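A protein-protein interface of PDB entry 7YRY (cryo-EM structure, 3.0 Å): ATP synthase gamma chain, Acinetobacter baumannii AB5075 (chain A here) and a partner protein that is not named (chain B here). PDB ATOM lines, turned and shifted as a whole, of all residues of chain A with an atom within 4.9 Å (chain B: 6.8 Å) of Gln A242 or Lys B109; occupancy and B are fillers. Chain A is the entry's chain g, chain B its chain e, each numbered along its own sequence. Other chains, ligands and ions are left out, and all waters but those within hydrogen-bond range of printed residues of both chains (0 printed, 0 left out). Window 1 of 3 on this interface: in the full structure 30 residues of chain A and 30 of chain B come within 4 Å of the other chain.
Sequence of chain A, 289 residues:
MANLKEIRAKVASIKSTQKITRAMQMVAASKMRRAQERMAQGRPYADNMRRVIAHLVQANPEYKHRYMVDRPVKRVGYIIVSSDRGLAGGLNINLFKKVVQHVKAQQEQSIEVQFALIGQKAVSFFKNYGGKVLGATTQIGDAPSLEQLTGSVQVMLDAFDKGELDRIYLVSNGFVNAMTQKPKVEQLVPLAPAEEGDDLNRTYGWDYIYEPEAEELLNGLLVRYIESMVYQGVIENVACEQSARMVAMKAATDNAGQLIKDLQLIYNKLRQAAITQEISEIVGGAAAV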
ATOM      1  N   ALA A  28     -23.284 -23.602  24.073  1.00  0.00           N
ATOM      2  CA  ALA A  28     -24.530 -24.358  24.034  1.00  0.00           C
ATOM      3  C   ALA A  28     -25.738 -23.432  24.075  1.00  0.00           C
ATOM      4  O   ALA A  28     -26.736 -23.675  23.392  1.00  0.00           O
ATOM      5  CB  ALA A  28     -24.575 -25.356  25.190  1.00  0.00           C
ATOM      6  N   LYS A  31     -26.129 -21.947  20.595  1.00  0.00           N
ATOM      7  CA  LYS A  31     -26.731 -22.925  19.693  1.00  0.00           C
ATOM      8  C   LYS A  31     -28.211 -23.117  19.999  1.00  0.00           C
ATOM      9  O   LYS A  31     -29.028 -23.277  19.083  1.00  0.00           O
ATOM     10  CB  LYS A  31     -25.983 -24.256  19.782  1.00  0.00           C
ATOM     11  CG  LYS A  31     -24.778 -24.346  18.864  1.00  0.00           C
ATOM     12  CD  LYS A  31     -23.939 -25.576  19.167  1.00  0.00           C
ATOM     13  CE  LYS A  31     -22.761 -25.678  18.210  1.00  0.00           C
ATOM     14  NZ  LYS A  31     -21.703 -26.591  18.720  1.00  0.00           N
ATOM     15  N   MET A  32     -28.571 -23.111  21.284  1.00  0.00           N
ATOM     16  CA  MET A  32     -29.970 -23.228  21.677  1.00  0.00           C
ATOM     17  C   MET A  32     -30.794 -22.077  21.118  1.00  0.00           C
ATOM     18  O   MET A  32     -31.885 -22.287  20.580  1.00  0.00           O
ATOM     19  CB  MET A  32     -30.077 -23.275  23.202  1.00  0.00           C
ATOM     20  CG  MET A  32     -31.442 -22.877  23.744  1.00  0.00           C
ATOM     21  SD  MET A  32     -31.343 -22.113  25.375  1.00  0.00           S
ATOM     22  CE  MET A  32     -32.803 -21.074  25.356  1.00  0.00           C
ATOM     23  N   ASN A 237     -37.209 -31.248  19.196  1.00  0.00           N
ATOM     24  CA  ASN A 237     -36.322 -32.015  20.062  1.00  0.00           C
ATOM     25  C   ASN A 237     -34.910 -31.450  20.055  1.00  0.00           C
ATOM     26  O   ASN A 237     -34.240 -31.440  21.091  1.00  0.00           O
ATOM     27  CB  ASN A 237     -36.304 -33.486  19.664  1.00  0.00           C
ATOM     28  CG  ASN A 237     -36.984 -34.358  20.688  1.00  0.00           C
ATOM     29  OD1 ASN A 237     -37.455 -33.868  21.708  1.00  0.00           O
ATOM     30  ND2 ASN A 237     -36.986 -35.658  20.458  1.00  0.00           N
ATOM     31  N   VAL A 238     -34.430 -30.995  18.898  1.00  0.00           N
ATOM     32  CA  VAL A 238     -33.100 -30.386  18.845  1.00  0.00           C
ATOM     33  C   VAL A 238     -33.057 -29.143  19.726  1.00  0.00           C
ATOM     34  O   VAL A 238     -32.126 -28.947  20.526  1.00  0.00           O
ATOM     35  CB  VAL A 238     -32.714 -30.066  17.388  1.00  0.00           C
ATOM     36  CG1 VAL A 238     -31.740 -28.901  17.330  1.00  0.00           C
ATOM     37  CG2 VAL A 238     -32.122 -31.293  16.718  1.00  0.00           C
ATOM     38  N   ALA A 239     -34.082 -28.294  19.609  1.00  0.00           N
ATOM     39  CA  ALA A 239     -34.141 -27.080  20.416  1.00  0.00           C
ATOM     40  C   ALA A 239     -34.179 -27.407  21.902  1.00  0.00           C
ATOM     41  O   ALA A 239     -33.495 -26.762  22.705  1.00  0.00           O
ATOM     42  CB  ALA A 239     -35.357 -26.242  20.018  1.00  0.00           C
ATOM     43  N   CYS A 240     -34.976 -28.405  22.290  1.00  0.00           N
ATOM     44  CA  CYS A 240     -35.065 -28.771  23.701  1.00  0.00           C
ATOM     45  C   CYS A 240     -33.760 -29.373  24.208  1.00  0.00           C
ATOM     46  O   CYS A 240     -33.322 -29.067  25.323  1.00  0.00           O
ATOM     47  CB  CYS A 240     -36.225 -29.741  23.918  1.00  0.00           C
ATOM     48  SG  CYS A 240     -36.822 -29.797  25.620  1.00  0.00           S
ATOM     49  N   GLU A 241     -33.128 -30.236  23.408  1.00  0.00           N
ATOM     50  CA  GLU A 241     -31.892 -30.888  23.827  1.00  0.00           C
ATOM     51  C   GLU A 241     -30.762 -29.886  24.004  1.00  0.00           C
ATOM     52  O   GLU A 241     -29.918 -30.058  24.891  1.00  0.00           O
ATOM     53  CB  GLU A 241     -31.516 -31.978  22.817  1.00  0.00           C
ATOM     54  CG  GLU A 241     -30.114 -32.566  22.966  1.00  0.00           C
ATOM     55  CD  GLU A 241     -29.077 -31.883  22.091  1.00  0.00           C
ATOM     56  OE1 GLU A 241     -29.320 -30.747  21.635  1.00  0.00           O
ATOM     57  OE2 GLU A 241     -28.010 -32.489  21.855  1.00  0.00           O
ATOM     58  N   GLN A 242     -30.729 -28.834  23.185  1.00  0.00           N
ATOM     59  CA  GLN A 242     -29.663 -27.848  23.331  1.00  0.00           C
ATOM     60  C   GLN A 242     -29.750 -27.046  24.627  1.00  0.00           C
ATOM     61  O   GLN A 242     -28.802 -26.319  24.942  1.00  0.00           O
ATOM     62  CB  GLN A 242     -29.659 -26.897  22.132  1.00  0.00           C
ATOM     63  CG  GLN A 242     -28.269 -26.583  21.594  1.00  0.00           C
ATOM     64  CD  GLN A 242     -27.579 -27.795  20.999  1.00  0.00           C
ATOM     65  OE1 GLN A 242     -28.181 -28.562  20.247  1.00  0.00           O
ATOM     66  NE2 GLN A 242     -26.306 -27.974  21.334  1.00  0.00           N
ATOM     67  N   SER A 243     -30.846 -27.151  25.380  1.00  0.00           N
ATOM     68  CA  SER A 243     -31.076 -26.306  26.547  1.00  0.00           C
ATOM     69  C   SER A 243     -30.697 -26.954  27.878  1.00  0.00           C
ATOM     70  O   SER A 243     -30.880 -26.322  28.924  1.00  0.00           O
ATOM     71  CB  SER A 243     -32.545 -25.875  26.594  1.00  0.00           C
ATOM     72  OG  SER A 243     -33.402 -26.999  26.684  1.00  0.00           O
ATOM     73  N   ALA A 244     -30.180 -28.185  27.877  1.00  0.00           N
ATOM     74  CA  ALA A 244     -29.782 -28.849  29.115  1.00  0.00           C
ATOM     75  C   ALA A 244     -28.272 -28.915  29.305  1.00  0.00           C
ATOM     76  O   ALA A 244     -27.799 -29.067  30.445  1.00  0.00           O
ATOM     77  CB  ALA A 244     -30.356 -30.271  29.162  1.00  0.00           C
ATOM     78  N   ARG A 245     -27.511 -28.803  28.214  1.00  0.00           N
ATOM     79  CA  ARG A 245     -26.060 -28.826  28.324  1.00  0.00           C
ATOM     80  C   ARG A 245     -25.565 -27.713  29.233  1.00  0.00           C
ATOM     81  O   ARG A 245     -24.704 -27.946  30.085  1.00  0.00           O
ATOM     82  CB  ARG A 245     -25.427 -28.713  26.937  1.00  0.00           C
ATOM     83  CG  ARG A 245     -25.891 -29.775  25.957  1.00  0.00           C
ATOM     84  CD  ARG A 245     -24.997 -29.812  24.728  1.00  0.00           C
ATOM     85  NE  ARG A 245     -25.083 -31.085  24.021  1.00  0.00           N
ATOM     86  CZ  ARG A 245     -24.284 -32.120  24.244  1.00  0.00           C
ATOM     87  NH1 ARG A 245     -23.325 -32.070  25.154  1.00  0.00           N
ATOM     88  NH2 ARG A 245     -24.450 -33.232  23.533  1.00  0.00           N
ATOM     89  N   GLN B 103     -21.658 -30.665   7.061  1.00  0.00           N
ATOM     90  CA  GLN B 103     -20.757 -31.740   7.461  1.00  0.00           C
ATOM     91  C   GLN B 103     -19.591 -31.198   8.275  1.00  0.00           C
ATOM     92  O   GLN B 103     -19.218 -31.776   9.305  1.00  0.00           O
ATOM     93  CB  GLN B 103     -20.252 -32.484   6.225  1.00  0.00           C
ATOM     94  CG  GLN B 103     -19.305 -33.634   6.527  1.00  0.00           C
ATOM     95  CD  GLN B 103     -19.953 -34.720   7.364  1.00  0.00           C
ATOM     96  OE1 GLN B 103     -19.463 -35.070   8.437  1.00  0.00           O
ATOM     97  NE2 GLN B 103     -21.059 -35.266   6.872  1.00  0.00           N
ATOM     98  N   LEU B 104     -19.007 -30.080   7.834  1.00  0.00           N
ATOM     99  CA  LEU B 104     -17.897 -29.484   8.567  1.00  0.00           C
ATOM    100  C   LEU B 104     -18.330 -29.029   9.952  1.00  0.00           C
ATOM    101  O   LEU B 104     -17.613 -29.250  10.932  1.00  0.00           O
ATOM    102  CB  LEU B 104     -17.313 -28.313   7.778  1.00  0.00           C
ATOM    103  CG  LEU B 104     -15.797 -28.137   7.883  1.00  0.00           C
ATOM    104  CD1 LEU B 104     -15.083 -29.458   7.643  1.00  0.00           C
ATOM    105  CD2 LEU B 104     -15.312 -27.074   6.912  1.00  0.00           C
ATOM    106  N   LEU B 105     -19.496 -28.386  10.057  1.00  0.00           N
ATOM    107  CA  LEU B 105     -19.952 -27.933  11.365  1.00  0.00           C
ATOM    108  C   LEU B 105     -20.200 -29.114  12.291  1.00  0.00           C
ATOM    109  O   LEU B 105     -19.852 -29.062  13.475  1.00  0.00           O
ATOM    110  CB  LEU B 105     -21.201 -27.053  11.223  1.00  0.00           C
ATOM    111  CG  LEU B 105     -22.616 -27.596  11.000  1.00  0.00           C
ATOM    112  CD1 LEU B 105     -23.290 -28.003  12.302  1.00  0.00           C
ATOM    113  CD2 LEU B 105     -23.458 -26.556  10.279  1.00  0.00           C
ATOM    114  N   ALA B 106     -20.785 -30.197  11.771  1.00  0.00           N
ATOM    115  CA  ALA B 106     -21.014 -31.375  12.600  1.00  0.00           C
ATOM    116  C   ALA B 106     -19.700 -31.981  13.080  1.00  0.00           C
ATOM    117  O   ALA B 106     -19.560 -32.326  14.262  1.00  0.00           O
ATOM    118  CB  ALA B 106     -21.831 -32.409  11.826  1.00  0.00           C
ATOM    119  N   ASN B 107     -18.722 -32.112  12.181  1.00  0.00           N
ATOM    120  CA  ASN B 107     -17.442 -32.703  12.563  1.00  0.00           C
ATOM    121  C   ASN B 107     -16.714 -31.838  13.588  1.00  0.00           C
ATOM    122  O   ASN B 107     -16.196 -32.347  14.593  1.00  0.00           O
ATOM    123  CB  ASN B 107     -16.577 -32.928  11.322  1.00  0.00           C
ATOM    124  CG  ASN B 107     -17.261 -33.794  10.282  1.00  0.00           C
ATOM    125  OD1 ASN B 107     -17.001 -33.667   9.085  1.00  0.00           O
ATOM    126  ND2 ASN B 107     -18.136 -34.685  10.733  1.00  0.00           N
ATOM    127  N   GLN B 108     -16.672 -30.522  13.357  1.00  0.00           N
ATOM    128  CA  GLN B 108     -16.029 -29.632  14.319  1.00  0.00           C
ATOM    129  C   GLN B 108     -16.752 -29.643  15.658  1.00  0.00           C
ATOM    130  O   GLN B 108     -16.106 -29.603  16.707  1.00  0.00           O
ATOM    131  CB  GLN B 108     -15.939 -28.201  13.777  1.00  0.00           C
ATOM    132  CG  GLN B 108     -15.284 -28.015  12.408  1.00  0.00           C
ATOM    133  CD  GLN B 108     -14.393 -29.172  11.996  1.00  0.00           C
ATOM    134  OE1 GLN B 108     -13.258 -29.289  12.461  1.00  0.00           O
ATOM    135  NE2 GLN B 108     -14.893 -30.019  11.105  1.00  0.00           N
ATOM    136  N   LYS B 109     -18.086 -29.690  15.650  1.00  0.00           N
ATOM    137  CA  LYS B 109     -18.825 -29.719  16.907  1.00  0.00           C
ATOM    138  C   LYS B 109     -18.535 -30.995  17.686  1.00  0.00           C
ATOM    139  O   LYS B 109     -18.352 -30.955  18.909  1.00  0.00           O
ATOM    140  CB  LYS B 109     -20.323 -29.575  16.639  1.00  0.00           C
ATOM    141  CG  LYS B 109     -21.195 -29.784  17.863  1.00  0.00           C
ATOM    142  CD  LYS B 109     -22.668 -29.685  17.509  1.00  0.00           C
ATOM    143  CE  LYS B 109     -23.546 -29.907  18.729  1.00  0.00           C
ATOM    144  NZ  LYS B 109     -24.990 -29.952  18.369  1.00  0.00           N
ATOM    145  N   SER B 110     -18.488 -32.138  16.996  1.00  0.00           N
ATOM    146  CA  SER B 110     -18.144 -33.385  17.674  1.00  0.00           C
ATOM    147  C   SER B 110     -16.740 -33.315  18.262  1.00  0.00           C
ATOM    148  O   SER B 110     -16.516 -33.724  19.411  1.00  0.00           O
ATOM    149  CB  SER B 110     -18.260 -34.562  16.707  1.00  0.00           C
ATOM    150  OG  SER B 110     -17.344 -34.432  15.633  1.00  0.00           O
ATOM    151  N   ASP B 111     -15.784 -32.789  17.491  1.00  0.00           N
ATOM    152  CA  ASP B 111     -14.414 -32.667  17.984  1.00  0.00           C
ATOM    153  C   ASP B 111     -14.351 -31.762  19.209  1.00  0.00           C
ATOM    154  O   ASP B 111     -13.685 -32.086  20.201  1.00  0.00           O
ATOM    155  CB  ASP B 111     -13.509 -32.135  16.872  1.00  0.00           C
ATOM    156  CG  ASP B 111     -12.079 -31.932  17.331  1.00  0.00           C
ATOM    157  OD1 ASP B 111     -11.621 -32.685  18.217  1.00  0.00           O
ATOM    158  OD2 ASP B 111     -11.412 -31.015  16.809  1.00  0.00           O
ATOM    159  N   LEU B 112     -15.040 -30.621  19.154  1.00  0.00           N
ATOM    160  CA  LEU B 112     -15.026 -29.683  20.271  1.00  0.00           C
ATOM    161  C   LEU B 112     -15.641 -30.304  21.516  1.00  0.00           C
ATOM    162  O   LEU B 112     -15.090 -30.188  22.615  1.00  0.00           O
ATOM    163  CB  LEU B 112     -15.766 -28.398  19.890  1.00  0.00           C
ATOM    164  CG  LEU B 112     -15.160 -27.560  18.763  1.00  0.00           C
ATOM    165  CD1 LEU B 112     -15.996 -26.316  18.503  1.00  0.00           C
ATOM    166  CD2 LEU B 112     -13.717 -27.196  19.073  1.00  0.00           C
ATOM    167  N   ASP B 113     -16.781 -30.982  21.361  1.00  0.00           N
ATOM    168  CA  ASP B 113     -17.425 -31.615  22.507  1.00  0.00           C
ATOM    169  C   ASP B 113     -16.511 -32.660  23.134  1.00  0.00           C
ATOM    170  O   ASP B 113     -16.294 -32.663  24.354  1.00  0.00           O
ATOM    171  CB  ASP B 113     -18.750 -32.244  22.076  1.00  0.00           C
ATOM    172  CG  ASP B 113     -19.616 -32.644  23.252  1.00  0.00           C
ATOM    173  OD1 ASP B 113     -20.321 -31.770  23.797  1.00  0.00           O
ATOM    174  OD2 ASP B 113     -19.594 -33.834  23.627  1.00  0.00           O
ATOM    175  N   SER B 114     -15.948 -33.544  22.304  1.00  0.00           N
ATOM    176  CA  SER B 114     -15.071 -34.590  22.819  1.00  0.00           C
ATOM    177  C   SER B 114     -13.877 -33.995  23.554  1.00  0.00           C
ATOM    178  O   SER B 114     -13.622 -34.328  24.718  1.00  0.00           O
ATOM    179  CB  SER B 114     -14.605 -35.489  21.674  1.00  0.00           C
ATOM    180  OG  SER B 114     -13.280 -35.939  21.890  1.00  0.00           O
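Of the 12 printed residues of chain B, 2 touch a printed residue of chain A.
Among the printed residues, 3 pairs touch across the chains.
Among the printed residues, Asp or Glu carboxylates within 4 Å of a Lys or Arg side-chain nitrogen of the other chain: Arg A245 with Asp B113 (3.3 Å).
CG of Lys B109 touches NZ of Lys A31, at 3.3 Å.
Lys B109 touches Gln A242 (NZ to NE2, 3.8 Å).
NH1 of Arg A245 is in salt-bridge range of OD1 of Asp B113.
The side-chain carboxylate of Glu A241 sits close to the side-chain amide oxygen of Gln A242.
The side-chain carboxylate (OE2) of Glu A241 lies within salt-bridge range of the guanidinium group (NE) of Arg A245, at 3.9 Å.
Of chain B, only Lys B109 comes within 4 Å of Gln A242.
Lys B109 touches two residues of chain A.
Printed residues of chain B within 4 Å of Lys A31: Lys B109.
Of the printed residues of chain A, Asp B113 touches Arg A245.
Printed residues of chain B within 4 Å of Arg A245: Asp B113.
Leu B105 touches none of the printed residues of chain A.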
